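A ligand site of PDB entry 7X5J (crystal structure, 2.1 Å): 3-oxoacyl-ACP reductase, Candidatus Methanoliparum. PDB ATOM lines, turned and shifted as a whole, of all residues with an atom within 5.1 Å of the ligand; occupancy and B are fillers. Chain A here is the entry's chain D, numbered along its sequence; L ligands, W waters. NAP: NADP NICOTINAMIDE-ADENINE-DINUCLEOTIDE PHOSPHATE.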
ATOM      1  N   GLY A  12       3.277   3.185  26.311  1.00  0.00           N
ATOM      2  CA  GLY A  12       2.924   4.546  25.843  1.00  0.00           C
ATOM      3  C   GLY A  12       4.029   5.187  25.015  1.00  0.00           C
ATOM      4  O   GLY A  12       4.178   6.424  25.094  1.00  0.00           O
ATOM      5  N   GLY A  13       4.728   4.402  24.192  1.00  0.00           N
ATOM      6  CA  GLY A  13       5.689   4.914  23.193  1.00  0.00           C
ATOM      7  C   GLY A  13       4.988   5.532  21.984  1.00  0.00           C
ATOM      8  O   GLY A  13       5.708   5.999  21.105  1.00  0.00           O
ATOM      9  N   SER A  14       3.649   5.577  21.967  1.00  0.00           N
ATOM     10  CA  SER A  14       2.808   6.103  20.853  1.00  0.00           C
ATOM     11  C   SER A  14       3.034   7.611  20.677  1.00  0.00           C
ATOM     12  O   SER A  14       2.924   8.089  19.539  1.00  0.00           O
ATOM     13  CB  SER A  14       1.341   5.808  21.077  1.00  0.00           C
ATOM     14  OG  SER A  14       0.724   6.795  21.896  1.00  0.00           O
ATOM     15  N   GLY A  15       3.291   8.329  21.765  1.00  0.00           N
ATOM     16  CA  GLY A  15       3.713   9.743  21.748  1.00  0.00           C
ATOM     17  C   GLY A  15       4.162  10.226  23.122  1.00  0.00           C
ATOM     18  O   GLY A  15       4.299   9.384  24.049  1.00  0.00           O
ATOM     19  N   GLY A  16       4.344  11.545  23.249  1.00  0.00           N
ATOM     20  CA  GLY A  16       4.784  12.225  24.475  1.00  0.00           C
ATOM     21  C   GLY A  16       6.201  11.820  24.856  1.00  0.00           C
ATOM     22  O   GLY A  16       7.008  11.585  23.947  1.00  0.00           O
ATOM     23  N   LEU A  17       6.478  11.727  26.160  1.00  0.00           N
ATOM     24  CA  LEU A  17       7.834  11.431  26.698  1.00  0.00           C
ATOM     25  C   LEU A  17       8.241  10.012  26.295  1.00  0.00           C
ATOM     26  O   LEU A  17       9.446   9.822  25.999  1.00  0.00           O
ATOM     27  CB  LEU A  17       7.817  11.599  28.219  1.00  0.00           C
ATOM     28  CG  LEU A  17       7.367  12.970  28.702  1.00  0.00           C
ATOM     29  CD1 LEU A  17       7.297  12.984  30.231  1.00  0.00           C
ATOM     30  CD2 LEU A  17       8.294  14.063  28.188  1.00  0.00           C
ATOM     31  N   GLY A  18       7.289   9.068  26.293  1.00  0.00           N
ATOM     32  CA  GLY A  18       7.513   7.657  25.905  1.00  0.00           C
ATOM     33  C   GLY A  18       8.181   7.536  24.545  1.00  0.00           C
ATOM     34  O   GLY A  18       9.149   6.755  24.426  1.00  0.00           O
ATOM     35  N   THR A  35       4.326   0.669  22.528  1.00  0.00           N
ATOM     36  CA  THR A  35       2.871   0.351  22.484  1.00  0.00           C
ATOM     37  C   THR A  35       2.077   1.538  21.940  1.00  0.00           C
ATOM     38  O   THR A  35       2.548   2.697  22.066  1.00  0.00           O
ATOM     39  CB  THR A  35       2.261  -0.072  23.831  1.00  0.00           C
ATOM     40  OG1 THR A  35       2.036   1.104  24.614  1.00  0.00           O
ATOM     41  CG2 THR A  35       3.111  -1.089  24.568  1.00  0.00           C
ATOM     42  N   GLY A  36       0.926   1.228  21.357  1.00  0.00           N
ATOM     43  CA  GLY A  36      -0.208   2.142  21.158  1.00  0.00           C
ATOM     44  C   GLY A  36      -1.452   1.528  21.771  1.00  0.00           C
ATOM     45  O   GLY A  36      -1.497   0.295  21.936  1.00  0.00           O
ATOM     46  N   ASN A  37      -2.418   2.364  22.143  1.00  0.00           N
ATOM     47  CA  ASN A  37      -3.754   1.907  22.598  1.00  0.00           C
ATOM     48  C   ASN A  37      -4.825   2.573  21.738  1.00  0.00           C
ATOM     49  O   ASN A  37      -5.431   1.855  20.925  1.00  0.00           O
ATOM     50  CB  ASN A  37      -3.957   2.136  24.094  1.00  0.00           C
ATOM     51  CG  ASN A  37      -5.214   1.470  24.594  1.00  0.00           C
ATOM     52  OD1 ASN A  37      -5.484   0.323  24.248  1.00  0.00           O
ATOM     53  ND2 ASN A  37      -5.984   2.181  25.397  1.00  0.00           N
ATOM     54  N   ARG A  38      -4.998   3.887  21.889  1.00  0.00           N
ATOM     55  CA  ARG A  38      -5.882   4.742  21.043  1.00  0.00           C
ATOM     56  C   ARG A  38      -5.138   5.193  19.777  1.00  0.00           C
ATOM     57  O   ARG A  38      -5.850   5.667  18.866  1.00  0.00           O
ATOM     58  CB  ARG A  38      -6.339   5.992  21.784  1.00  0.00           C
ATOM     59  CG  ARG A  38      -7.087   5.735  23.092  1.00  0.00           C
ATOM     60  CD  ARG A  38      -8.575   5.496  22.909  1.00  0.00           C
ATOM     61  NE  ARG A  38      -9.142   4.876  24.103  1.00  0.00           N
ATOM     62  CZ  ARG A  38      -9.421   5.507  25.244  1.00  0.00           C
ATOM     63  NH1 ARG A  38      -9.219   6.804  25.370  1.00  0.00           N
ATOM     64  NH2 ARG A  38      -9.915   4.820  26.256  1.00  0.00           N
ATOM     65  N   ASN A  39      -3.805   5.065  19.720  1.00  0.00           N
ATOM     66  CA  ASN A  39      -2.951   5.690  18.655  1.00  0.00           C
ATOM     67  C   ASN A  39      -1.887   4.724  18.119  1.00  0.00           C
ATOM     68  O   ASN A  39      -0.706   5.126  18.055  1.00  0.00           O
ATOM     69  CB  ASN A  39      -2.287   6.973  19.149  1.00  0.00           C
ATOM     70  CG  ASN A  39      -3.284   8.091  19.354  1.00  0.00           C
ATOM     71  OD1 ASN A  39      -3.744   8.715  18.396  1.00  0.00           O
ATOM     72  ND2 ASN A  39      -3.628   8.355  20.600  1.00  0.00           N
ATOM     73  N   ILE A  40      -2.297   3.532  17.677  1.00  0.00           N
ATOM     74  CA  ILE A  40      -1.427   2.469  17.083  1.00  0.00           C
ATOM     75  C   ILE A  40      -0.667   3.005  15.855  1.00  0.00           C
ATOM     76  O   ILE A  40       0.485   2.564  15.638  1.00  0.00           O
ATOM     77  CB  ILE A  40      -2.268   1.230  16.726  1.00  0.00           C
ATOM     78  CG1 ILE A  40      -1.407   0.006  16.404  1.00  0.00           C
ATOM     79  CG2 ILE A  40      -3.231   1.555  15.583  1.00  0.00           C
ATOM     80  CD1 ILE A  40      -0.381  -0.321  17.459  1.00  0.00           C
ATOM     81  N   VAL A  62      -1.601  -2.448  22.711  1.00  0.00           N
ATOM     82  CA  VAL A  62      -1.753  -2.947  24.113  1.00  0.00           C
ATOM     83  C   VAL A  62      -2.520  -1.922  24.940  1.00  0.00           C
ATOM     84  O   VAL A  62      -2.127  -0.739  24.946  1.00  0.00           O
ATOM     85  CB  VAL A  62      -0.388  -3.245  24.775  1.00  0.00           C
ATOM     86  CG1 VAL A  62      -0.593  -3.964  26.103  1.00  0.00           C
ATOM     87  CG2 VAL A  62       0.547  -4.036  23.868  1.00  0.00           C
ATOM     88  N   ASP A  63      -3.566  -2.389  25.616  1.00  0.00           N
ATOM     89  CA  ASP A  63      -4.135  -1.754  26.833  1.00  0.00           C
ATOM     90  C   ASP A  63      -3.457  -2.447  28.020  1.00  0.00           C
ATOM     91  O   ASP A  63      -3.882  -3.579  28.345  1.00  0.00           O
ATOM     92  CB  ASP A  63      -5.651  -1.911  26.881  1.00  0.00           C
ATOM     93  CG  ASP A  63      -6.305  -1.283  28.103  1.00  0.00           C
ATOM     94  OD1 ASP A  63      -5.570  -0.858  29.030  1.00  0.00           O
ATOM     95  OD2 ASP A  63      -7.553  -1.246  28.107  1.00  0.00           O
ATOM     96  N   VAL A  64      -2.451  -1.800  28.607  1.00  0.00           N
ATOM     97  CA  VAL A  64      -1.562  -2.392  29.660  1.00  0.00           C
ATOM     98  C   VAL A  64      -2.396  -2.949  30.829  1.00  0.00           C
ATOM     99  O   VAL A  64      -1.875  -3.859  31.521  1.00  0.00           O
ATOM    100  CB  VAL A  64      -0.465  -1.412  30.125  1.00  0.00           C
ATOM    101  CG1 VAL A  64       0.540  -1.118  29.028  1.00  0.00           C
ATOM    102  CG2 VAL A  64      -1.029  -0.107  30.684  1.00  0.00           C
ATOM    103  N   SER A  65      -3.646  -2.489  31.040  1.00  0.00           N
ATOM    104  CA  SER A  65      -4.563  -3.025  32.077  1.00  0.00           C
ATOM    105  C   SER A  65      -5.048  -4.445  31.739  1.00  0.00           C
ATOM    106  O   SER A  65      -5.408  -5.192  32.684  1.00  0.00           O
ATOM    107  CB  SER A  65      -5.757  -2.138  32.293  1.00  0.00           C
ATOM    108  OG  SER A  65      -6.504  -1.980  31.093  1.00  0.00           O
ATOM    109  N   ASN A  89       7.627   1.390  32.055  1.00  0.00           N
ATOM    110  CA  ASN A  89       6.177   1.481  32.363  1.00  0.00           C
ATOM    111  C   ASN A  89       5.728   2.940  32.307  1.00  0.00           C
ATOM    112  O   ASN A  89       5.446   3.510  33.374  1.00  0.00           O
ATOM    113  CB  ASN A  89       5.891   0.875  33.742  1.00  0.00           C
ATOM    114  CG  ASN A  89       5.810  -0.634  33.669  1.00  0.00           C
ATOM    115  OD1 ASN A  89       5.124  -1.171  32.806  1.00  0.00           O
ATOM    116  ND2 ASN A  89       6.503  -1.309  34.573  1.00  0.00           N
ATOM    117  N   ASN A  90       5.617   3.502  31.095  1.00  0.00           N
ATOM    118  CA  ASN A  90       5.443   4.962  30.888  1.00  0.00           C
ATOM    119  C   ASN A  90       3.974   5.302  30.596  1.00  0.00           C
ATOM    120  O   ASN A  90       3.585   6.474  30.818  1.00  0.00           O
ATOM    121  CB  ASN A  90       6.436   5.465  29.831  1.00  0.00           C
ATOM    122  CG  ASN A  90       5.989   6.715  29.111  1.00  0.00           C
ATOM    123  OD1 ASN A  90       6.419   7.808  29.450  1.00  0.00           O
ATOM    124  ND2 ASN A  90       5.144   6.545  28.105  1.00  0.00           N
ATOM    125  N   ALA A  91       3.169   4.331  30.154  1.00  0.00           N
ATOM    126  CA  ALA A  91       1.709   4.531  29.928  1.00  0.00           C
ATOM    127  C   ALA A  91       1.043   5.010  31.227  1.00  0.00           C
ATOM    128  O   ALA A  91       1.293   4.375  32.280  1.00  0.00           O
ATOM    129  CB  ALA A  91       1.070   3.248  29.432  1.00  0.00           C
ATOM    130  N   ALA A  92       0.225   6.068  31.147  1.00  0.00           N
ATOM    131  CA  ALA A  92      -0.541   6.615  32.297  1.00  0.00           C
ATOM    132  C   ALA A  92      -1.915   7.165  31.883  1.00  0.00           C
ATOM    133  O   ALA A  92      -2.020   7.841  30.853  1.00  0.00           O
ATOM    134  CB  ALA A  92       0.258   7.701  32.984  1.00  0.00           C
ATOM    135  N   SER A  93      -2.918   6.938  32.735  1.00  0.00           N
ATOM    136  CA  SER A  93      -4.282   7.518  32.673  1.00  0.00           C
ATOM    137  C   SER A  93      -4.475   8.489  33.844  1.00  0.00           C
ATOM    138  O   SER A  93      -3.925   8.231  34.933  1.00  0.00           O
ATOM    139  CB  SER A  93      -5.322   6.419  32.717  1.00  0.00           C
ATOM    140  OG  SER A  93      -6.580   6.926  33.154  1.00  0.00           O
ATOM    141  N   ILE A  95      -3.710  11.769  33.934  1.00  0.00           N
ATOM    142  CA  ILE A  95      -2.470  12.548  34.137  1.00  0.00           C
ATOM    143  C   ILE A  95      -2.803  13.973  34.595  1.00  0.00           C
ATOM    144  O   ILE A  95      -1.974  14.555  35.346  1.00  0.00           O
ATOM    145  CB  ILE A  95      -1.559  12.558  32.899  1.00  0.00           C
ATOM    146  CG1 ILE A  95      -1.124  11.147  32.490  1.00  0.00           C
ATOM    147  CG2 ILE A  95      -0.358  13.461  33.165  1.00  0.00           C
ATOM    148  CD1 ILE A  95      -0.138  11.115  31.331  1.00  0.00           C
ATOM    149  N   VAL A 115      -4.667   1.268  34.870  1.00  0.00           N
ATOM    150  CA  VAL A 115      -3.620   1.650  33.886  1.00  0.00           C
ATOM    151  C   VAL A 115      -2.291   1.868  34.618  1.00  0.00           C
ATOM    152  O   VAL A 115      -1.256   1.311  34.167  1.00  0.00           O
ATOM    153  CB  VAL A 115      -4.058   2.867  33.062  1.00  0.00           C
ATOM    154  CG1 VAL A 115      -2.960   3.299  32.105  1.00  0.00           C
ATOM    155  CG2 VAL A 115      -5.348   2.595  32.308  1.00  0.00           C
ATOM    156  N   ILE A 142       7.658   5.069  36.005  1.00  0.00           N
ATOM    157  CA  ILE A 142       7.517   6.552  35.850  1.00  0.00           C
ATOM    158  C   ILE A 142       6.579   7.034  36.955  1.00  0.00           C
ATOM    159  O   ILE A 142       5.372   6.695  36.882  1.00  0.00           O
ATOM    160  CB  ILE A 142       7.041   6.919  34.425  1.00  0.00           C
ATOM    161  CG1 ILE A 142       7.994   6.364  33.355  1.00  0.00           C
ATOM    162  CG2 ILE A 142       6.859   8.419  34.265  1.00  0.00           C
ATOM    163  CD1 ILE A 142       9.420   6.875  33.442  1.00  0.00           C
ATOM    164  N   SER A 143       7.132   7.741  37.935  1.00  0.00           N
ATOM    165  CA  SER A 143       6.404   8.397  39.049  1.00  0.00           C
ATOM    166  C   SER A 143       6.402   9.915  38.827  1.00  0.00           C
ATOM    167  O   SER A 143       6.823  10.362  37.732  1.00  0.00           O
ATOM    168  CB  SER A 143       7.013   8.033  40.388  1.00  0.00           C
ATOM    169  OG  SER A 143       6.159   8.379  41.471  1.00  0.00           O
ATOM    170  N   SER A 144       5.973  10.687  39.823  1.00  0.00           N
ATOM    171  CA  SER A 144       5.734  12.150  39.730  1.00  0.00           C
ATOM    172  C   SER A 144       5.814  12.746  41.129  1.00  0.00           C
ATOM    173  O   SER A 144       5.347  12.106  42.066  1.00  0.00           O
ATOM    174  CB  SER A 144       4.388  12.430  39.050  1.00  0.00           C
ATOM    175  OG  SER A 144       3.791  13.645  39.500  1.00  0.00           O
ATOM    176  N   TYR A 157      -3.969  10.203  40.607  1.00  0.00           N
ATOM    177  CA  TYR A 157      -2.597  10.385  40.051  1.00  0.00           C
ATOM    178  C   TYR A 157      -1.574  10.290  41.199  1.00  0.00           C
ATOM    179  O   TYR A 157      -0.634   9.501  41.085  1.00  0.00           O
ATOM    180  CB  TYR A 157      -2.473  11.713  39.338  1.00  0.00           C
ATOM    181  CG  TYR A 157      -1.237  11.837  38.498  1.00  0.00           C
ATOM    182  CD1 TYR A 157      -1.024  10.980  37.425  1.00  0.00           C
ATOM    183  CD2 TYR A 157      -0.272  12.786  38.780  1.00  0.00           C
ATOM    184  CE1 TYR A 157       0.118  11.092  36.642  1.00  0.00           C
ATOM    185  CE2 TYR A 157       0.879  12.892  38.019  1.00  0.00           C
ATOM    186  CZ  TYR A 157       1.072  12.043  36.944  1.00  0.00           C
ATOM    187  OH  TYR A 157       2.190  12.183  36.169  1.00  0.00           O
ATOM    188  N   LYS A 161       1.046   7.254  41.411  1.00  0.00           N
ATOM    189  CA  LYS A 161       2.457   7.651  41.192  1.00  0.00           C
ATOM    190  C   LYS A 161       3.253   7.321  42.459  1.00  0.00           C
ATOM    191  O   LYS A 161       4.415   6.927  42.319  1.00  0.00           O
ATOM    192  CB  LYS A 161       2.527   9.105  40.746  1.00  0.00           C
ATOM    193  CG  LYS A 161       1.879   9.353  39.382  1.00  0.00           C
ATOM    194  CD  LYS A 161       2.660   8.780  38.218  1.00  0.00           C
ATOM    195  CE  LYS A 161       1.799   7.982  37.280  1.00  0.00           C
ATOM    196  NZ  LYS A 161       2.523   7.673  36.030  1.00  0.00           N
ATOM    197  N   LEU A 187       9.222  12.457  38.210  1.00  0.00           N
ATOM    198  CA  LEU A 187       9.237  13.573  37.220  1.00  0.00           C
ATOM    199  C   LEU A 187       8.697  14.854  37.873  1.00  0.00           C
ATOM    200  O   LEU A 187       7.735  14.766  38.655  1.00  0.00           O
ATOM    201  CB  LEU A 187       8.371  13.198  36.011  1.00  0.00           C
ATOM    202  CG  LEU A 187       9.014  12.309  34.935  1.00  0.00           C
ATOM    203  CD1 LEU A 187       9.558  11.013  35.536  1.00  0.00           C
ATOM    204  CD2 LEU A 187       8.013  12.005  33.836  1.00  0.00           C
ATOM    205  N   GLY A 188       9.281  15.991  37.538  1.00  0.00           N
ATOM    206  CA  GLY A 188       8.620  17.305  37.624  1.00  0.00           C
ATOM    207  C   GLY A 188       7.717  17.497  36.419  1.00  0.00           C
ATOM    208  O   GLY A 188       6.938  16.585  36.091  1.00  0.00           O
ATOM    209  N   VAL A 189       7.871  18.635  35.741  1.00  0.00           N
ATOM    210  CA  VAL A 189       7.031  18.976  34.550  1.00  0.00           C
ATOM    211  C   VAL A 189       7.958  19.144  33.350  1.00  0.00           C
ATOM    212  O   VAL A 189       9.109  19.602  33.534  1.00  0.00           O
ATOM    213  CB  VAL A 189       6.176  20.225  34.831  1.00  0.00           C
ATOM    214  CG1 VAL A 189       5.188  19.941  35.942  1.00  0.00           C
ATOM    215  CG2 VAL A 189       7.010  21.450  35.155  1.00  0.00           C
ATOM    216  N   PHE A 190       7.470  18.740  32.165  1.00  0.00           N
ATOM    217  CA  PHE A 190       8.273  18.697  30.916  1.00  0.00           C
ATOM    218  C   PHE A 190       7.570  19.503  29.807  1.00  0.00           C
ATOM    219  O   PHE A 190       6.352  19.397  29.679  1.00  0.00           O
ATOM    220  CB  PHE A 190       8.572  17.230  30.605  1.00  0.00           C
ATOM    221  CG  PHE A 190       9.570  16.654  31.577  1.00  0.00           C
ATOM    222  CD1 PHE A 190      10.933  16.773  31.340  1.00  0.00           C
ATOM    223  CD2 PHE A 190       9.157  16.106  32.789  1.00  0.00           C
ATOM    224  CE1 PHE A 190      11.862  16.300  32.258  1.00  0.00           C
ATOM    225  CE2 PHE A 190      10.091  15.655  33.707  1.00  0.00           C
ATOM    226  CZ  PHE A 190      11.443  15.752  33.441  1.00  0.00           C
ATOM    227  N   ARG A 195       1.788  19.965  22.986  1.00  0.00           N
ATOM    228  CA  ARG A 195       1.001  18.785  23.456  1.00  0.00           C
ATOM    229  C   ARG A 195       1.575  17.478  22.878  1.00  0.00           C
ATOM    230  O   ARG A 195       1.344  16.430  23.495  1.00  0.00           O
ATOM    231  CB  ARG A 195      -0.479  18.934  23.088  1.00  0.00           C
ATOM    232  CG  ARG A 195      -1.388  17.872  23.680  1.00  0.00           C
ATOM    233  CD  ARG A 195      -1.352  17.811  25.206  1.00  0.00           C
ATOM    234  NE  ARG A 195      -1.870  16.559  25.734  1.00  0.00           N
ATOM    235  CZ  ARG A 195      -1.152  15.450  25.910  1.00  0.00           C
ATOM    236  NH1 ARG A 195       0.147  15.414  25.598  1.00  0.00           N
ATOM    237  NH2 ARG A 195      -1.719  14.380  26.415  1.00  0.00           N
ATOM    238  N   ASP A 197       4.754  16.491  22.660  1.00  0.00           N
ATOM    239  CA  ASP A 197       5.908  16.003  23.469  1.00  0.00           C
ATOM    240  C   ASP A 197       5.534  15.841  24.947  1.00  0.00           C
ATOM    241  O   ASP A 197       6.271  15.098  25.616  1.00  0.00           O
ATOM    242  CB  ASP A 197       7.117  16.935  23.348  1.00  0.00           C
ATOM    243  CG  ASP A 197       7.905  16.762  22.068  1.00  0.00           C
ATOM    244  OD1 ASP A 197       7.958  15.634  21.554  1.00  0.00           O
ATOM    245  OD2 ASP A 197       8.495  17.757  21.602  1.00  0.00           O
ATOM    246  N   SER A 198       4.462  16.488  25.446  1.00  0.00           N
ATOM    247  CA  SER A 198       4.137  16.547  26.903  1.00  0.00           C
ATOM    248  C   SER A 198       2.644  16.751  27.175  1.00  0.00           C
ATOM    249  O   SER A 198       1.993  17.586  26.504  1.00  0.00           O
ATOM    250  CB  SER A 198       4.948  17.613  27.583  1.00  0.00           C
ATOM    251  OG  SER A 198       4.737  17.558  28.992  1.00  0.00           O
ATOM    252  N   SER A 199       2.138  16.040  28.199  1.00  0.00           N
ATOM    253  CA  SER A 199       0.801  16.231  28.803  1.00  0.00           C
ATOM    254  C   SER A 199       0.840  17.367  29.843  1.00  0.00           C
ATOM    255  O   SER A 199      -0.203  17.622  30.482  1.00  0.00           O
ATOM    256  CB  SER A 199       0.298  14.957  29.420  1.00  0.00           C
ATOM    257  OG  SER A 199       1.018  14.643  30.602  1.00  0.00           O
ATOM    258  N   PHE A 200       1.991  18.047  30.010  1.00  0.00           N
ATOM    259  CA  PHE A 200       2.027  19.327  30.757  1.00  0.00           C
ATOM    260  C   PHE A 200       1.098  20.334  30.071  1.00  0.00           C
ATOM    261  O   PHE A 200       0.521  21.190  30.765  1.00  0.00           O
ATOM    262  CB  PHE A 200       3.462  19.865  30.857  1.00  0.00           C
ATOM    263  CG  PHE A 200       3.644  21.103  31.702  1.00  0.00           C
ATOM    264  CD1 PHE A 200       3.050  21.219  32.955  1.00  0.00           C
ATOM    265  CD2 PHE A 200       4.500  22.122  31.289  1.00  0.00           C
ATOM    266  CE1 PHE A 200       3.234  22.358  33.728  1.00  0.00           C
ATOM    267  CE2 PHE A 200       4.697  23.250  32.077  1.00  0.00           C
ATOM    268  CZ  PHE A 200       4.067  23.362  33.289  1.00  0.00           C
HETATM  269  PA  NAP L   1       0.665  11.589  27.223  1.00  0.00           P
HETATM  270  O1A NAP L   1      -0.771  11.704  27.612  1.00  0.00           O
HETATM  271  O2A NAP L   1       1.228  12.598  26.286  1.00  0.00           O
HETATM  272  O5B NAP L   1       0.958  10.111  26.719  1.00  0.00           O
HETATM  273  C5B NAP L   1       0.165   9.094  27.384  1.00  0.00           C
HETATM  274  C4B NAP L   1       0.521   7.743  26.829  1.00  0.00           C
HETATM  275  O4B NAP L   1      -0.131   6.718  27.632  1.00  0.00           O
HETATM  276  C3B NAP L   1       0.091   7.485  25.366  1.00  0.00           C
HETATM  277  O3B NAP L   1       1.204   6.994  24.640  1.00  0.00           O
HETATM  278  C2B NAP L   1      -1.041   6.470  25.491  1.00  0.00           C
HETATM  279  O2B NAP L   1      -1.143   5.509  24.427  1.00  0.00           O
HETATM  280  C1B NAP L   1      -0.596   5.724  26.741  1.00  0.00           C
HETATM  281  N9A NAP L   1      -1.655   4.975  27.379  1.00  0.00           N
HETATM  282  C8A NAP L   1      -2.703   5.494  28.102  1.00  0.00           C
HETATM  283  N7A NAP L   1      -3.518   4.588  28.558  1.00  0.00           N
HETATM  284  C5A NAP L   1      -2.969   3.382  28.132  1.00  0.00           C
HETATM  285  C6A NAP L   1      -3.365   2.052  28.310  1.00  0.00           C
HETATM  286  N6A NAP L   1      -4.450   1.698  29.005  1.00  0.00           N
HETATM  287  N1A NAP L   1      -2.598   1.083  27.759  1.00  0.00           N
HETATM  288  C2A NAP L   1      -1.495   1.462  27.081  1.00  0.00           C
HETATM  289  N3A NAP L   1      -1.036   2.685  26.824  1.00  0.00           N
HETATM  290  C4A NAP L   1      -1.822   3.614  27.396  1.00  0.00           C
HETATM  291  O3  NAP L   1       1.547  11.611  28.565  1.00  0.00           O
HETATM  292  PN  NAP L   1       3.092  11.943  28.719  1.00  0.00           P
HETATM  293  O1N NAP L   1       3.199  13.423  28.879  1.00  0.00           O
HETATM  294  O2N NAP L   1       3.820  11.255  27.615  1.00  0.00           O
HETATM  295  O5D NAP L   1       3.441  11.221  30.119  1.00  0.00           O
HETATM  296  C5D NAP L   1       4.129   9.951  30.120  1.00  0.00           C
HETATM  297  C4D NAP L   1       4.436   9.525  31.537  1.00  0.00           C
HETATM  298  O4D NAP L   1       5.129  10.600  32.222  1.00  0.00           O
HETATM  299  C3D NAP L   1       3.224   9.178  32.392  1.00  0.00           C
HETATM  300  O3D NAP L   1       3.456   8.017  33.186  1.00  0.00           O
HETATM  301  C2D NAP L   1       3.052  10.425  33.266  1.00  0.00           C
HETATM  302  O2D NAP L   1       2.403  10.086  34.481  1.00  0.00           O
HETATM  303  C1D NAP L   1       4.489  10.861  33.453  1.00  0.00           C
HETATM  304  N1N NAP L   1       4.627  12.299  33.750  1.00  0.00           N
HETATM  305  C2N NAP L   1       4.606  13.206  32.723  1.00  0.00           C
HETATM  306  C3N NAP L   1       4.803  14.569  32.996  1.00  0.00           C
HETATM  307  C7N NAP L   1       4.916  15.593  31.893  1.00  0.00           C
HETATM  308  O7N NAP L   1       5.268  16.731  32.177  1.00  0.00           O
HETATM  309  N7N NAP L   1       4.657  15.220  30.645  1.00  0.00           N
HETATM  310  C4N NAP L   1       4.897  14.982  34.337  1.00  0.00           C
HETATM  311  C5N NAP L   1       4.993  14.032  35.324  1.00  0.00           C
HETATM  312  C6N NAP L   1       4.798  12.713  35.019  1.00  0.00           C
HETATM  313  P2B NAP L   1      -2.197   5.803  23.212  1.00  0.00           P
HETATM  314  O1X NAP L   1      -3.621   5.734  23.727  1.00  0.00           O
HETATM  315  O2X NAP L   1      -1.801   7.188  22.689  1.00  0.00           O
HETATM  316  O3X NAP L   1      -1.907   4.711  22.200  1.00  0.00           O
HETATM  317  O   HOH W   1      -3.498   8.562  23.705  1.00  0.00           O
HETATM  318  O   HOH W   2      -6.789   3.848  29.621  1.00  0.00           O
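The side-chain carboxylate (OD1) of Asp 63 is in hydrogen-bond range of the side-chain hydroxyl (OG) of Ser 65 (2.5 Å). The side-chain hydroxyl of Thr 35 is in hydrogen-bond range of the backbone NH of Gly 12. The side-chain amino group (NZ) of Lys 161 sits at hydrogen-bond distance from the backbone carbonyl oxygen (O) of Ile 142, 3.1 Å away. The backbone NH (N) of Leu 187 is in hydrogen-bond range of the backbone carbonyl oxygen (O) of Ser 143, at 3.2 Å. The backbone carbonyl oxygen (O) of Thr 35 lies within hydrogen-bond range of the backbone NH (N) of Ser 14. The backbone carbonyl oxygen of Ser 198 is in hydrogen-bond range of the guanidinium group of Arg 195 (3.0 Å). N of Leu 17 is in hydrogen-bond range of O of Asp 197. The backbone NH (N) of Phe 200 sits at hydrogen-bond distance from the side-chain hydroxyl (OG) of Ser 198, at 3.0 Å.
Water W1 bridges O2X of the ligand (2.4 Å) and ND2 of Asn 39 (3.1 Å).
A nitrogen (N7N) of the ligand is in hydrogen-bond range of the side-chain hydroxyl (OG) of Ser 198 (2.9 Å). N of Leu 17 lies within hydrogen-bond range of O2N of the ligand, at 3.1 Å. N of Ser 199 is in hydrogen-bond range of O1N of the ligand. The backbone NH (N) of Asn 37 lies within hydrogen-bond range of an oxygen (O3X) of the ligand. NH2 of Arg 195 lies within salt-bridge range of O1A of the ligand, at 3.1 Å. O of Gly 12 sits at hydrogen-bond distance from O3B of the ligand, 3.1 Å away. O2D of the ligand is in hydrogen-bond range of OH of Tyr 157. The side-chain amide nitrogen (ND2) of Asn 39 sits at hydrogen-bond distance from an oxygen (O2X) of the ligand (3.0 Å). The side-chain amino group of Lys 161 lies within hydrogen-bond range of an oxygen (O2D) of the ligand. An oxygen (O2X) of the ligand sits at hydrogen-bond distance from the side-chain hydroxyl (OG) of Ser 14 (2.7 Å). The backbone NH of Arg 38 lies within hydrogen-bond range of an oxygen (O1X) of the ligand (2.9 Å). The backbone NH (N) of Phe 190 sits at hydrogen-bond distance from an oxygen (O7N) of the ligand, at 3.0 Å. An oxygen (O3D) of the ligand lies within hydrogen-bond range of the backbone carbonyl oxygen (O) of Asn 90. OG of Ser 199 lies within hydrogen-bond range of O1N of the ligand (3.0 Å). The backbone NH (N) of Asn 39 is in hydrogen-bond range of an oxygen (O3X) of the ligand (3.1 Å). OD1 of Asp 63 sits at hydrogen-bond distance from N6A of the ligand (2.8 Å). N1A of the ligand is in hydrogen-bond range of N of Val 64 (3.0 Å).
N1A of the ligand sits close to O of Val 62 (3.4 Å). Residues that only touch the ligand: Gly 188 (3.1 Å), Ala 92 (3.2 Å), Gly 36 (3.2 Å), Ile 95 (3.3 Å), Ala 91 (3.4 Å), Leu 187 (3.4 Å), Gly 16 (3.4 Å), Ile 142 (3.5 Å), Val 115 (3.5 Å), Val 189 (3.7 Å), Gly 15 (3.8 Å) and Phe 200 (3.9 Å). Of the 38 residues printed, 28 come within 4 Å of the ligand. The nearest printed residue that does not touch the ligand is Ser 144 (4.1 Å).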
